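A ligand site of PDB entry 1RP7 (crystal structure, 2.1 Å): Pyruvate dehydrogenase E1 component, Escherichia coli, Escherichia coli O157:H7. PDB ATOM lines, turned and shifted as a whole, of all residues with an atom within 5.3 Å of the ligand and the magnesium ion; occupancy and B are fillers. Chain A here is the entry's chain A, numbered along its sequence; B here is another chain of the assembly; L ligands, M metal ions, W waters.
Of the 33 residues printed, 3 come within 4 Å of the magnesium ion.
An oxygen (O7) of the ligand lies within hydrogen-bond range of a ring nitrogen (NE2) of His 142 (2.6 Å).
An oxygen (O7) of the ligand lies within hydrogen-bond range of the side-chain hydroxyl (OG) of Ser 109 (2.7 Å).
An oxygen (O6) of the ligand lies within hydrogen-bond range of the side-chain amide nitrogen (NE2) of Gln 140 (3.2 Å).
A nitrogen (N1) of the ligand lies within hydrogen-bond range of the side-chain carboxylate (OE2) of Glu 571 of chain B (2.8 Å).
An oxygen (O4) of the ligand lies close to the backbone NH of Asp 230 (3.5 Å).
N of Met 194 lies close to N2 of the ligand, 3.2 Å away.
The side-chain amino group of Lys 392 lies within salt-bridge range of an oxygen (O7) of the ligand (3.7 Å).
The backbone carbonyl oxygen (O) of Val 192 is in hydrogen-bond range of a nitrogen (N3) of the ligand (2.6 Å).
O5 of the ligand is in hydrogen-bond range of N of Glu 232, 3.0 Å away.
N of Gly 231 sits close to O4 of the ligand.
The side-chain hydroxyl of Ser 112 is in hydrogen-bond range of the side-chain amide nitrogen of Asn 258 (3.1 Å).
OE1 of Glu 235 is in salt-bridge range of NH2 of Arg 606 of chain B, at 3.5 Å.
OD2 of Asp 230 sits at hydrogen-bond distance from N of Leu 261 (2.7 Å).
The side-chain carboxylate (OD2) of Asp 521 of chain B lies within hydrogen-bond range of the backbone NH (N) of Leu 264, at 2.8 Å.
OE1 of Glu 571 of chain B sits close to OE2 of Glu 235 (2.5 Å).
OG of Ser 193 sits at hydrogen-bond distance from NH1 of Arg 606 of chain B, at 2.8 Å.
The side-chain amide nitrogen (ND2) of Asn 260 lies within hydrogen-bond range of the side-chain hydroxyl (OG) of Ser 112 (3.2 Å).
OG of Ser 112 lies within hydrogen-bond range of O of Ser 109.
O of Gln 262 binds the magnesium ion.
The magnesium ion is bound by OD1 of Asp 230.
The side-chain amide oxygen (OD1) of Asn 260 is bound to the magnesium ion (2.3 Å).
The magnesium ion is bound by O8 of the ligand, 2.3 Å away.
Water W2 binds the magnesium ion.
O4 of the ligand binds the magnesium ion (2.3 Å).
The magnesium ion has six donor atoms within binding distance.
Water W2 lies within hydrogen-bond range of an oxygen (O6) of the ligand, the backbone carbonyl oxygen of Asn 258, the backbone NH of Asp 230 and the side-chain amide nitrogen of Asn 260.
Water W4 lies within hydrogen-bond range of O5 of the ligand (2.7 Å), NE2 of Gln 140 (2.9 Å), OE1 of Glu 232 (3.0 Å), SD of Met 194 (3.4 Å) and N of Gly 229 (3.5 Å).
Water W1 lies within hydrogen-bond range of OE1 of Glu 636 of chain B, NE2 of His 640 of chain B and O1 of the ligand.
Water W3 lies within hydrogen-bond range of OE1 of Gln 140 (2.5 Å), OG of Ser 109 (2.7 Å), ND2 of Asn 258 (3.0 Å) and O6 of the ligand (3.3 Å).
The side-chain carboxylate of Glu 522 of chain B lies close to a nitrogen (N4) of the ligand (3.5 Å).
Residues that only touch the ligand: Asp 521 of chain B (3.2 Å), Glu 235 (3.3 Å), Gly 229 (3.3 Å), Arg 606 of chain B (3.5 Å), Ile 569 of chain B (3.5 Å), His 640 of chain B (3.5 Å), Ser 193 (3.6 Å), Arg 263 (3.6 Å), Phe 602 of chain B (3.7 Å), Leu 264 (3.7 Å) and Asn 258 (3.8 Å).
Hydrophobic or aromatic side chains that line the ligand: His 142, Met 194, Leu 264, Ile 569 of chain B, Phe 602 of chain B and His 640 of chain B.
Within 4 Å of the ligand: Ser 109, Gln 140, His 142, Val 192, Ser 193, Met 194, Gly 229, Asp 230, Gly 231, Glu 232, Glu 235, Asn 258, Asn 260, Gln 262, Arg 263, Leu 264, Lys 392, Asp 521 of chain B, Glu 522 of chain B, Ile 569 of chain B, Glu 571 of chain B, Phe 602 of chain B, Arg 606 of chain B and His 640 of chain B.
The nearest printed residue that does not touch the ligand is Tyr 599 of chain B (4.005 Å).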
ATOM      1  N   HIS A 106     -23.317  -1.240 -14.909  1.00  0.00           N
ATOM      2  CA  HIS A 106     -23.624  -0.614 -13.635  1.00  0.00           C
ATOM      3  C   HIS A 106     -24.761  -1.297 -12.882  1.00  0.00           C
ATOM      4  O   HIS A 106     -25.549  -2.028 -13.469  1.00  0.00           O
ATOM      5  CB  HIS A 106     -23.960   0.873 -13.860  1.00  0.00           C
ATOM      6  CG  HIS A 106     -22.968   1.581 -14.729  1.00  0.00           C
ATOM      7  ND1 HIS A 106     -22.269   2.696 -14.315  1.00  0.00           N
ATOM      8  CD2 HIS A 106     -22.529   1.308 -15.977  1.00  0.00           C
ATOM      9  CE1 HIS A 106     -21.451   3.081 -15.276  1.00  0.00           C
ATOM     10  NE2 HIS A 106     -21.584   2.255 -16.289  1.00  0.00           N
ATOM     11  N   SER A 109     -26.860   2.543  -9.745  1.00  0.00           N
ATOM     12  CA  SER A 109     -27.711   3.573 -10.306  1.00  0.00           C
ATOM     13  C   SER A 109     -29.145   3.109 -10.513  1.00  0.00           C
ATOM     14  O   SER A 109     -30.074   3.751 -10.020  1.00  0.00           O
ATOM     15  CB  SER A 109     -27.144   4.074 -11.628  1.00  0.00           C
ATOM     16  OG  SER A 109     -27.699   5.331 -11.932  1.00  0.00           O
ATOM     17  N   SER A 112     -31.207   2.900  -7.461  1.00  0.00           N
ATOM     18  CA  SER A 112     -31.779   4.106  -6.894  1.00  0.00           C
ATOM     19  C   SER A 112     -32.994   4.610  -7.686  1.00  0.00           C
ATOM     20  O   SER A 112     -33.802   5.363  -7.163  1.00  0.00           O
ATOM     21  CB  SER A 112     -30.710   5.208  -6.793  1.00  0.00           C
ATOM     22  OG  SER A 112     -30.293   5.700  -8.054  1.00  0.00           O
ATOM     23  N   GLN A 140     -32.190   6.713 -18.925  1.00  0.00           N
ATOM     24  CA  GLN A 140     -30.824   7.011 -18.547  1.00  0.00           C
ATOM     25  C   GLN A 140     -30.030   5.840 -19.120  1.00  0.00           C
ATOM     26  O   GLN A 140     -30.387   4.684 -18.929  1.00  0.00           O
ATOM     27  CB  GLN A 140     -30.689   7.040 -17.037  1.00  0.00           C
ATOM     28  CG  GLN A 140     -29.425   7.682 -16.561  1.00  0.00           C
ATOM     29  CD  GLN A 140     -29.412   7.784 -15.060  1.00  0.00           C
ATOM     30  OE1 GLN A 140     -30.249   7.176 -14.384  1.00  0.00           O
ATOM     31  NE2 GLN A 140     -28.470   8.540 -14.523  1.00  0.00           N
ATOM     32  N   HIS A 142     -27.000   4.254 -18.543  1.00  0.00           N
ATOM     33  CA  HIS A 142     -26.405   3.208 -17.729  1.00  0.00           C
ATOM     34  C   HIS A 142     -27.314   2.420 -16.798  1.00  0.00           C
ATOM     35  O   HIS A 142     -26.832   1.664 -15.949  1.00  0.00           O
ATOM     36  CB  HIS A 142     -25.211   3.766 -16.936  1.00  0.00           C
ATOM     37  CG  HIS A 142     -25.528   5.004 -16.151  1.00  0.00           C
ATOM     38  ND1 HIS A 142     -25.970   6.174 -16.736  1.00  0.00           N
ATOM     39  CD2 HIS A 142     -25.405   5.274 -14.826  1.00  0.00           C
ATOM     40  CE1 HIS A 142     -26.091   7.111 -15.817  1.00  0.00           C
ATOM     41  NE2 HIS A 142     -25.758   6.587 -14.639  1.00  0.00           N
ATOM     42  N   TYR A 177     -25.337   0.196 -23.685  1.00  0.00           N
ATOM     43  CA  TYR A 177     -26.277   1.289 -23.578  1.00  0.00           C
ATOM     44  C   TYR A 177     -27.235   1.426 -24.758  1.00  0.00           C
ATOM     45  O   TYR A 177     -27.125   0.692 -25.744  1.00  0.00           O
ATOM     46  CB  TYR A 177     -25.492   2.589 -23.394  1.00  0.00           C
ATOM     47  CG  TYR A 177     -24.355   2.477 -22.396  1.00  0.00           C
ATOM     48  CD1 TYR A 177     -24.616   2.167 -21.064  1.00  0.00           C
ATOM     49  CD2 TYR A 177     -23.029   2.698 -22.788  1.00  0.00           C
ATOM     50  CE1 TYR A 177     -23.575   2.091 -20.130  1.00  0.00           C
ATOM     51  CE2 TYR A 177     -21.988   2.622 -21.853  1.00  0.00           C
ATOM     52  CZ  TYR A 177     -22.274   2.325 -20.527  1.00  0.00           C
ATOM     53  OH  TYR A 177     -21.279   2.293 -19.577  1.00  0.00           O
ATOM     54  N   VAL A 192     -26.252   7.706 -23.347  1.00  0.00           N
ATOM     55  CA  VAL A 192     -25.060   7.649 -22.492  1.00  0.00           C
ATOM     56  C   VAL A 192     -24.136   8.832 -22.557  1.00  0.00           C
ATOM     57  O   VAL A 192     -23.412   9.073 -21.595  1.00  0.00           O
ATOM     58  CB  VAL A 192     -24.169   6.418 -22.685  1.00  0.00           C
ATOM     59  CG1 VAL A 192     -24.365   5.486 -21.517  1.00  0.00           C
ATOM     60  CG2 VAL A 192     -24.388   5.762 -24.025  1.00  0.00           C
ATOM     61  N   SER A 193     -24.099   9.561 -23.663  1.00  0.00           N
ATOM     62  CA  SER A 193     -23.224  10.721 -23.643  1.00  0.00           C
ATOM     63  C   SER A 193     -24.053  11.752 -22.921  1.00  0.00           C
ATOM     64  O   SER A 193     -24.917  12.402 -23.516  1.00  0.00           O
ATOM     65  CB  SER A 193     -22.886  11.230 -25.044  1.00  0.00           C
ATOM     66  OG  SER A 193     -22.026  12.340 -24.935  1.00  0.00           O
ATOM     67  N   MET A 194     -23.811  11.893 -21.616  1.00  0.00           N
ATOM     68  CA  MET A 194     -24.550  12.829 -20.793  1.00  0.00           C
ATOM     69  C   MET A 194     -24.703  14.207 -21.427  1.00  0.00           C
ATOM     70  O   MET A 194     -23.806  14.684 -22.125  1.00  0.00           O
ATOM     71  CB  MET A 194     -23.884  12.973 -19.421  1.00  0.00           C
ATOM     72  CG  MET A 194     -23.142  11.763 -18.923  1.00  0.00           C
ATOM     73  SD  MET A 194     -24.027  10.811 -17.700  1.00  0.00           S
ATOM     74  CE  MET A 194     -25.145  10.000 -18.765  1.00  0.00           C
ATOM     75  N   GLY A 229     -29.603  12.228 -14.650  1.00  0.00           N
ATOM     76  CA  GLY A 229     -28.931  12.046 -13.389  1.00  0.00           C
ATOM     77  C   GLY A 229     -28.654  13.455 -12.888  1.00  0.00           C
ATOM     78  O   GLY A 229     -28.675  14.369 -13.702  1.00  0.00           O
ATOM     79  N   ASP A 230     -28.418  13.658 -11.600  1.00  0.00           N
ATOM     80  CA  ASP A 230     -28.155  15.016 -11.146  1.00  0.00           C
ATOM     81  C   ASP A 230     -26.732  15.448 -11.498  1.00  0.00           C
ATOM     82  O   ASP A 230     -26.467  16.629 -11.696  1.00  0.00           O
ATOM     83  CB  ASP A 230     -28.401  15.177  -9.630  1.00  0.00           C
ATOM     84  CG  ASP A 230     -27.937  13.983  -8.818  1.00  0.00           C
ATOM     85  OD1 ASP A 230     -27.361  13.046  -9.405  1.00  0.00           O
ATOM     86  OD2 ASP A 230     -28.158  13.972  -7.595  1.00  0.00           O
ATOM     87  N   GLY A 231     -25.825  14.482 -11.573  1.00  0.00           N
ATOM     88  CA  GLY A 231     -24.455  14.789 -11.930  1.00  0.00           C
ATOM     89  C   GLY A 231     -24.417  15.281 -13.369  1.00  0.00           C
ATOM     90  O   GLY A 231     -23.686  16.209 -13.706  1.00  0.00           O
ATOM     91  N   GLU A 232     -25.211  14.632 -14.227  1.00  0.00           N
ATOM     92  CA  GLU A 232     -25.318  14.943 -15.646  1.00  0.00           C
ATOM     93  C   GLU A 232     -25.816  16.372 -15.923  1.00  0.00           C
ATOM     94  O   GLU A 232     -25.471  16.958 -16.956  1.00  0.00           O
ATOM     95  CB  GLU A 232     -26.263  13.940 -16.320  1.00  0.00           C
ATOM     96  CG  GLU A 232     -26.815  14.386 -17.660  1.00  0.00           C
ATOM     97  CD  GLU A 232     -27.629  13.323 -18.333  1.00  0.00           C
ATOM     98  OE1 GLU A 232     -28.314  12.557 -17.607  1.00  0.00           O
ATOM     99  OE2 GLU A 232     -27.613  13.224 -19.576  1.00  0.00           O
ATOM    100  N   GLU A 235     -23.540  19.148 -17.168  1.00  0.00           N
ATOM    101  CA  GLU A 235     -23.195  19.320 -18.564  1.00  0.00           C
ATOM    102  C   GLU A 235     -23.946  20.577 -18.994  1.00  0.00           C
ATOM    103  O   GLU A 235     -25.118  20.723 -18.670  1.00  0.00           O
ATOM    104  CB  GLU A 235     -23.657  18.130 -19.415  1.00  0.00           C
ATOM    105  CG  GLU A 235     -22.911  16.816 -19.148  1.00  0.00           C
ATOM    106  CD  GLU A 235     -21.512  16.784 -19.770  1.00  0.00           C
ATOM    107  OE1 GLU A 235     -21.007  17.869 -20.151  1.00  0.00           O
ATOM    108  OE2 GLU A 235     -20.924  15.688 -19.867  1.00  0.00           O
ATOM    109  N   ASN A 258     -32.942  12.158 -11.461  1.00  0.00           N
ATOM    110  CA  ASN A 258     -32.762  11.262 -10.329  1.00  0.00           C
ATOM    111  C   ASN A 258     -31.755  11.929  -9.406  1.00  0.00           C
ATOM    112  O   ASN A 258     -30.559  11.951  -9.677  1.00  0.00           O
ATOM    113  CB  ASN A 258     -32.247   9.917 -10.816  1.00  0.00           C
ATOM    114  CG  ASN A 258     -32.071   8.934  -9.682  1.00  0.00           C
ATOM    115  OD1 ASN A 258     -32.430   9.220  -8.542  1.00  0.00           O
ATOM    116  ND2 ASN A 258     -31.517   7.764  -9.996  1.00  0.00           N
ATOM    117  N   ASN A 260     -29.874  11.477  -6.534  1.00  0.00           N
ATOM    118  CA  ASN A 260     -29.318  10.629  -5.481  1.00  0.00           C
ATOM    119  C   ASN A 260     -28.109  11.321  -4.873  1.00  0.00           C
ATOM    120  O   ASN A 260     -27.336  10.733  -4.108  1.00  0.00           O
ATOM    121  CB  ASN A 260     -28.977   9.216  -5.996  1.00  0.00           C
ATOM    122  CG  ASN A 260     -28.164   9.254  -7.266  1.00  0.00           C
ATOM    123  OD1 ASN A 260     -27.402  10.177  -7.473  1.00  0.00           O
ATOM    124  ND2 ASN A 260     -28.316   8.236  -8.097  1.00  0.00           N
ATOM    125  N   LEU A 261     -27.960  12.601  -5.225  1.00  0.00           N
ATOM    126  CA  LEU A 261     -26.904  13.484  -4.721  1.00  0.00           C
ATOM    127  C   LEU A 261     -25.470  13.133  -5.082  1.00  0.00           C
ATOM    128  O   LEU A 261     -24.538  13.837  -4.675  1.00  0.00           O
ATOM    129  CB  LEU A 261     -27.027  13.613  -3.204  1.00  0.00           C
ATOM    130  CG  LEU A 261     -28.439  13.810  -2.624  1.00  0.00           C
ATOM    131  CD1 LEU A 261     -28.392  13.766  -1.104  1.00  0.00           C
ATOM    132  CD2 LEU A 261     -28.994  15.146  -3.095  1.00  0.00           C
ATOM    133  N   GLN A 262     -25.280  12.048  -5.824  1.00  0.00           N
ATOM    134  CA  GLN A 262     -23.929  11.657  -6.192  1.00  0.00           C
ATOM    135  C   GLN A 262     -23.743  11.469  -7.689  1.00  0.00           C
ATOM    136  O   GLN A 262     -24.684  11.127  -8.402  1.00  0.00           O
ATOM    137  CB  GLN A 262     -23.535  10.356  -5.485  1.00  0.00           C
ATOM    138  CG  GLN A 262     -24.421   9.907  -4.340  1.00  0.00           C
ATOM    139  CD  GLN A 262     -24.078   8.505  -3.838  1.00  0.00           C
ATOM    140  OE1 GLN A 262     -24.886   7.865  -3.147  1.00  0.00           O
ATOM    141  NE2 GLN A 262     -22.884   8.027  -4.174  1.00  0.00           N
ATOM    142  N   ARG A 263     -22.525  11.707  -8.165  1.00  0.00           N
ATOM    143  CA  ARG A 263     -22.214  11.461  -9.562  1.00  0.00           C
ATOM    144  C   ARG A 263     -21.333  10.216  -9.546  1.00  0.00           C
ATOM    145  O   ARG A 263     -21.542   9.331  -8.726  1.00  0.00           O
ATOM    146  CB  ARG A 263     -21.496  12.653 -10.200  1.00  0.00           C
ATOM    147  CG  ARG A 263     -20.623  13.450  -9.290  1.00  0.00           C
ATOM    148  CD  ARG A 263     -20.007  14.576 -10.081  1.00  0.00           C
ATOM    149  NE  ARG A 263     -19.360  15.544  -9.218  1.00  0.00           N
ATOM    150  CZ  ARG A 263     -18.238  15.324  -8.554  1.00  0.00           C
ATOM    151  NH1 ARG A 263     -17.613  14.159  -8.681  1.00  0.00           N
ATOM    152  NH2 ARG A 263     -17.733  16.269  -7.792  1.00  0.00           N
ATOM    153  N   LEU A 264     -20.349  10.130 -10.438  1.00  0.00           N
ATOM    154  CA  LEU A 264     -19.497   8.948 -10.467  1.00  0.00           C
ATOM    155  C   LEU A 264     -18.521   8.902  -9.304  1.00  0.00           C
ATOM    156  O   LEU A 264     -18.594   8.012  -8.455  1.00  0.00           O
ATOM    157  CB  LEU A 264     -18.733   8.868 -11.779  1.00  0.00           C
ATOM    158  CG  LEU A 264     -18.496   7.495 -12.417  1.00  0.00           C
ATOM    159  CD1 LEU A 264     -17.150   6.958 -11.967  1.00  0.00           C
ATOM    160  CD2 LEU A 264     -19.617   6.530 -12.053  1.00  0.00           C
ATOM    161  N   VAL A 268     -22.590  15.464  -6.235  1.00  0.00           N
ATOM    162  CA  VAL A 268     -22.638  16.585  -7.171  1.00  0.00           C
ATOM    163  C   VAL A 268     -22.100  17.838  -6.467  1.00  0.00           C
ATOM    164  O   VAL A 268     -21.096  18.416  -6.892  1.00  0.00           O
ATOM    165  CB  VAL A 268     -24.085  16.801  -7.677  1.00  0.00           C
ATOM    166  CG1 VAL A 268     -24.095  17.728  -8.877  1.00  0.00           C
ATOM    167  CG2 VAL A 268     -24.690  15.462  -8.081  1.00  0.00           C
ATOM    168  N   LYS A 392     -28.300   6.140  -3.945  1.00  0.00           N
ATOM    169  CA  LYS A 392     -27.489   5.404  -4.915  1.00  0.00           C
ATOM    170  C   LYS A 392     -27.015   4.102  -4.272  1.00  0.00           C
ATOM    171  O   LYS A 392     -26.512   4.113  -3.146  1.00  0.00           O
ATOM    172  CB  LYS A 392     -26.285   6.246  -5.346  1.00  0.00           C
ATOM    173  CG  LYS A 392     -25.660   5.796  -6.654  1.00  0.00           C
ATOM    174  CD  LYS A 392     -24.750   6.855  -7.227  1.00  0.00           C
ATOM    175  CE  LYS A 392     -24.529   6.640  -8.720  1.00  0.00           C
ATOM    176  NZ  LYS A 392     -23.478   7.546  -9.288  1.00  0.00           N
ATOM    177  N   ASP A 609     -20.506  15.693 -31.123  1.00  0.00           N
ATOM    178  CA  ASP A 609     -20.968  14.575 -30.315  1.00  0.00           C
ATOM    179  C   ASP A 609     -22.427  14.238 -30.654  1.00  0.00           C
ATOM    180  O   ASP A 609     -22.835  13.090 -30.567  1.00  0.00           O
ATOM    181  CB  ASP A 609     -20.817  14.895 -28.828  1.00  0.00           C
ATOM    182  CG  ASP A 609     -20.569  13.655 -27.995  1.00  0.00           C
ATOM    183  OD1 ASP A 609     -20.098  12.629 -28.537  1.00  0.00           O
ATOM    184  OD2 ASP A 609     -20.834  13.699 -26.776  1.00  0.00           O
ATOM    185  N   ALA B 520     -13.031  15.434 -14.987  1.00  0.00           N
ATOM    186  CA  ALA B 520     -14.450  15.671 -15.125  1.00  0.00           C
ATOM    187  C   ALA B 520     -15.141  14.488 -14.479  1.00  0.00           C
ATOM    188  O   ALA B 520     -15.533  13.541 -15.146  1.00  0.00           O
ATOM    189  CB  ALA B 520     -14.821  15.769 -16.604  1.00  0.00           C
ATOM    190  N   ASP B 521     -15.265  14.555 -13.159  1.00  0.00           N
ATOM    191  CA  ASP B 521     -15.899  13.519 -12.344  1.00  0.00           C
ATOM    192  C   ASP B 521     -15.013  12.280 -12.163  1.00  0.00           C
ATOM    193  O   ASP B 521     -14.395  12.118 -11.102  1.00  0.00           O
ATOM    194  CB  ASP B 521     -17.248  13.096 -12.947  1.00  0.00           C
ATOM    195  CG  ASP B 521     -18.083  12.281 -11.976  1.00  0.00           C
ATOM    196  OD1 ASP B 521     -17.746  12.270 -10.778  1.00  0.00           O
ATOM    197  OD2 ASP B 521     -19.082  11.669 -12.416  1.00  0.00           O
ATOM    198  N   GLU B 522     -14.968  11.442 -13.200  1.00  0.00           N
ATOM    199  CA  GLU B 522     -14.169  10.220 -13.195  1.00  0.00           C
ATOM    200  C   GLU B 522     -12.698  10.462 -12.868  1.00  0.00           C
ATOM    201  O   GLU B 522     -12.004  11.225 -13.533  1.00  0.00           O
ATOM    202  CB  GLU B 522     -14.242   9.537 -14.555  1.00  0.00           C
ATOM    203  CG  GLU B 522     -15.053   8.251 -14.568  1.00  0.00           C
ATOM    204  CD  GLU B 522     -16.546   8.503 -14.608  1.00  0.00           C
ATOM    205  OE1 GLU B 522     -16.995   9.488 -13.973  1.00  0.00           O
ATOM    206  OE2 GLU B 522     -17.271   7.718 -15.266  1.00  0.00           O
ATOM    207  N   ILE B 569     -19.332  16.151 -14.226  1.00  0.00           N
ATOM    208  CA  ILE B 569     -19.693  15.731 -15.587  1.00  0.00           C
ATOM    209  C   ILE B 569     -19.959  16.997 -16.392  1.00  0.00           C
ATOM    210  O   ILE B 569     -21.108  17.394 -16.610  1.00  0.00           O
ATOM    211  CB  ILE B 569     -20.940  14.816 -15.570  1.00  0.00           C
ATOM    212  CG1 ILE B 569     -20.786  13.765 -14.451  1.00  0.00           C
ATOM    213  CG2 ILE B 569     -21.118  14.138 -16.918  1.00  0.00           C
ATOM    214  CD1 ILE B 569     -22.029  12.932 -14.211  1.00  0.00           C
ATOM    215  N   GLU B 571     -17.517  18.302 -19.491  1.00  0.00           N
ATOM    216  CA  GLU B 571     -16.296  18.325 -20.298  1.00  0.00           C
ATOM    217  C   GLU B 571     -15.951  19.717 -20.785  1.00  0.00           C
ATOM    218  O   GLU B 571     -14.786  20.095 -20.820  1.00  0.00           O
ATOM    219  CB  GLU B 571     -16.435  17.367 -21.492  1.00  0.00           C
ATOM    220  CG  GLU B 571     -16.199  15.894 -21.131  1.00  0.00           C
ATOM    221  CD  GLU B 571     -17.422  15.249 -20.510  1.00  0.00           C
ATOM    222  OE1 GLU B 571     -18.517  15.830 -20.638  1.00  0.00           O
ATOM    223  OE2 GLU B 571     -17.287  14.175 -19.900  1.00  0.00           O
ATOM    224  N   TYR B 599     -12.443  10.833 -20.775  1.00  0.00           N
ATOM    225  CA  TYR B 599     -12.723   9.762 -21.724  1.00  0.00           C
ATOM    226  C   TYR B 599     -12.494  10.396 -23.085  1.00  0.00           C
ATOM    227  O   TYR B 599     -13.276  11.257 -23.513  1.00  0.00           O
ATOM    228  CB  TYR B 599     -14.165   9.310 -21.608  1.00  0.00           C
ATOM    229  CG  TYR B 599     -14.496   8.579 -20.329  1.00  0.00           C
ATOM    230  CD1 TYR B 599     -14.863   9.282 -19.184  1.00  0.00           C
ATOM    231  CD2 TYR B 599     -14.464   7.197 -20.276  1.00  0.00           C
ATOM    232  CE1 TYR B 599     -15.199   8.605 -18.009  1.00  0.00           C
ATOM    233  CE2 TYR B 599     -14.802   6.512 -19.106  1.00  0.00           C
ATOM    234  CZ  TYR B 599     -15.167   7.226 -17.980  1.00  0.00           C
ATOM    235  OH  TYR B 599     -15.525   6.559 -16.828  1.00  0.00           O
ATOM    236  N   PHE B 602     -14.977  12.056 -25.496  1.00  0.00           N
ATOM    237  CA  PHE B 602     -15.611  13.308 -25.149  1.00  0.00           C
ATOM    238  C   PHE B 602     -14.662  14.498 -25.140  1.00  0.00           C
ATOM    239  O   PHE B 602     -14.861  15.466 -24.403  1.00  0.00           O
ATOM    240  CB  PHE B 602     -16.326  13.165 -23.803  1.00  0.00           C
ATOM    241  CG  PHE B 602     -17.228  11.962 -23.737  1.00  0.00           C
ATOM    242  CD1 PHE B 602     -18.191  11.740 -24.711  1.00  0.00           C
ATOM    243  CD2 PHE B 602     -17.071  11.006 -22.735  1.00  0.00           C
ATOM    244  CE1 PHE B 602     -18.973  10.602 -24.702  1.00  0.00           C
ATOM    245  CE2 PHE B 602     -17.855   9.857 -22.707  1.00  0.00           C
ATOM    246  CZ  PHE B 602     -18.804   9.654 -23.699  1.00  0.00           C
ATOM    247  N   ARG B 606     -16.668  16.396 -28.552  1.00  0.00           N
ATOM    248  CA  ARG B 606     -17.626  17.083 -27.716  1.00  0.00           C
ATOM    249  C   ARG B 606     -17.329  18.557 -27.431  1.00  0.00           C
ATOM    250  O   ARG B 606     -18.247  19.348 -27.246  1.00  0.00           O
ATOM    251  CB  ARG B 606     -17.780  16.309 -26.390  1.00  0.00           C
ATOM    252  CG  ARG B 606     -18.693  16.982 -25.397  1.00  0.00           C
ATOM    253  CD  ARG B 606     -20.126  16.938 -25.869  1.00  0.00           C
ATOM    254  NE  ARG B 606     -21.051  17.258 -24.795  1.00  0.00           N
ATOM    255  CZ  ARG B 606     -21.722  16.352 -24.091  1.00  0.00           C
ATOM    256  NH1 ARG B 606     -21.579  15.057 -24.343  1.00  0.00           N
ATOM    257  NH2 ARG B 606     -22.525  16.752 -23.117  1.00  0.00           N
ATOM    258  N   GLU B 636     -17.739  -0.630 -23.127  1.00  0.00           N
ATOM    259  CA  GLU B 636     -18.530   0.589 -23.273  1.00  0.00           C
ATOM    260  C   GLU B 636     -19.315   0.792 -24.562  1.00  0.00           C
ATOM    261  O   GLU B 636     -20.388   1.393 -24.535  1.00  0.00           O
ATOM    262  CB  GLU B 636     -17.637   1.794 -22.997  1.00  0.00           C
ATOM    263  CG  GLU B 636     -17.129   1.814 -21.569  1.00  0.00           C
ATOM    264  CD  GLU B 636     -18.260   1.776 -20.532  1.00  0.00           C
ATOM    265  OE1 GLU B 636     -19.008   2.770 -20.455  1.00  0.00           O
ATOM    266  OE2 GLU B 636     -18.383   0.779 -19.798  1.00  0.00           O
ATOM    267  N   HIS B 640     -18.612   5.457 -26.744  1.00  0.00           N
ATOM    268  CA  HIS B 640     -17.431   5.577 -25.909  1.00  0.00           C
ATOM    269  C   HIS B 640     -16.149   5.146 -26.613  1.00  0.00           C
ATOM    270  O   HIS B 640     -15.086   5.714 -26.399  1.00  0.00           O
ATOM    271  CB  HIS B 640     -17.584   4.703 -24.661  1.00  0.00           C
ATOM    272  CG  HIS B 640     -18.461   5.287 -23.605  1.00  0.00           C
ATOM    273  ND1 HIS B 640     -19.833   5.154 -23.609  1.00  0.00           N
ATOM    274  CD2 HIS B 640     -18.151   5.947 -22.465  1.00  0.00           C
ATOM    275  CE1 HIS B 640     -20.324   5.700 -22.516  1.00  0.00           C
ATOM    276  NE2 HIS B 640     -19.330   6.195 -21.803  1.00  0.00           N
HETATM  277  N1  LIG L   1     -19.260  12.138 -19.833  1.00  0.00           N
HETATM  278  C1  LIG L   1     -20.220  11.896 -20.797  1.00  0.00           C
HETATM  279  C2  LIG L   1     -20.494  12.992 -21.758  1.00  0.00           C
HETATM  280  N2  LIG L   1     -20.889  10.747 -20.875  1.00  0.00           N
HETATM  281  C3  LIG L   1     -20.612   9.730 -19.962  1.00  0.00           C
HETATM  282  N3  LIG L   1     -21.280   8.612 -20.110  1.00  0.00           N
HETATM  283  C4  LIG L   1     -19.598   9.946 -18.908  1.00  0.00           C
HETATM  284  C5  LIG L   1     -18.960  11.161 -18.899  1.00  0.00           C
HETATM  285  C6  LIG L   1     -19.191   8.902 -17.887  1.00  0.00           C
HETATM  286  N4  LIG L   1     -20.258   8.560 -16.872  1.00  0.00           N
HETATM  287  C7  LIG L   1     -21.069   7.478 -16.996  1.00  0.00           C
HETATM  288  O1  LIG L   1     -21.097   6.668 -17.937  1.00  0.00           O
HETATM  289  S1  LIG L   1     -22.124   7.362 -15.596  1.00  0.00           S
HETATM  290  C8  LIG L   1     -21.447   8.790 -14.900  1.00  0.00           C
HETATM  291  C9  LIG L   1     -20.458   9.326 -15.687  1.00  0.00           C
HETATM  292  C10 LIG L   1     -19.625  10.545 -15.399  1.00  0.00           C
HETATM  293  C11 LIG L   1     -22.003   9.358 -13.625  1.00  0.00           C
HETATM  294  C12 LIG L   1     -23.500   9.513 -13.685  1.00  0.00           C
HETATM  295  O2  LIG L   1     -23.891  10.429 -12.633  1.00  0.00           O
HETATM  296  P1  LIG L   1     -25.365  11.048 -12.583  1.00  0.00           P
HETATM  297  O3  LIG L   1     -26.304   9.758 -12.514  1.00  0.00           O
HETATM  298  O4  LIG L   1     -25.484  11.815 -11.327  1.00  0.00           O
HETATM  299  O5  LIG L   1     -25.646  11.734 -13.874  1.00  0.00           O
HETATM  300  P2  LIG L   1     -26.468   8.528 -11.499  1.00  0.00           P
HETATM  301  O6  LIG L   1     -28.006   8.303 -11.377  1.00  0.00           O
HETATM  302  O7  LIG L   1     -25.850   7.336 -12.155  1.00  0.00           O
HETATM  303  O8  LIG L   1     -25.911   8.951 -10.197  1.00  0.00           O
HETATM  304 MG    MG M   1     -26.584  11.001  -9.426  1.00  0.00          MG
HETATM  305  O   HOH W   1     -18.523   5.134 -19.253  1.00  0.00           O
HETATM  306  O   HOH W   2     -28.539  10.620 -10.623  1.00  0.00           O
HETATM  307  O   HOH W   3     -30.286   6.060 -12.112  1.00  0.00           O
HETATM  308  O   HOH W   4     -26.887  10.489 -15.975  1.00  0.00           O
HETATM  309  O   HOH W   5     -17.551  13.356 -17.280  1.00  0.00           O
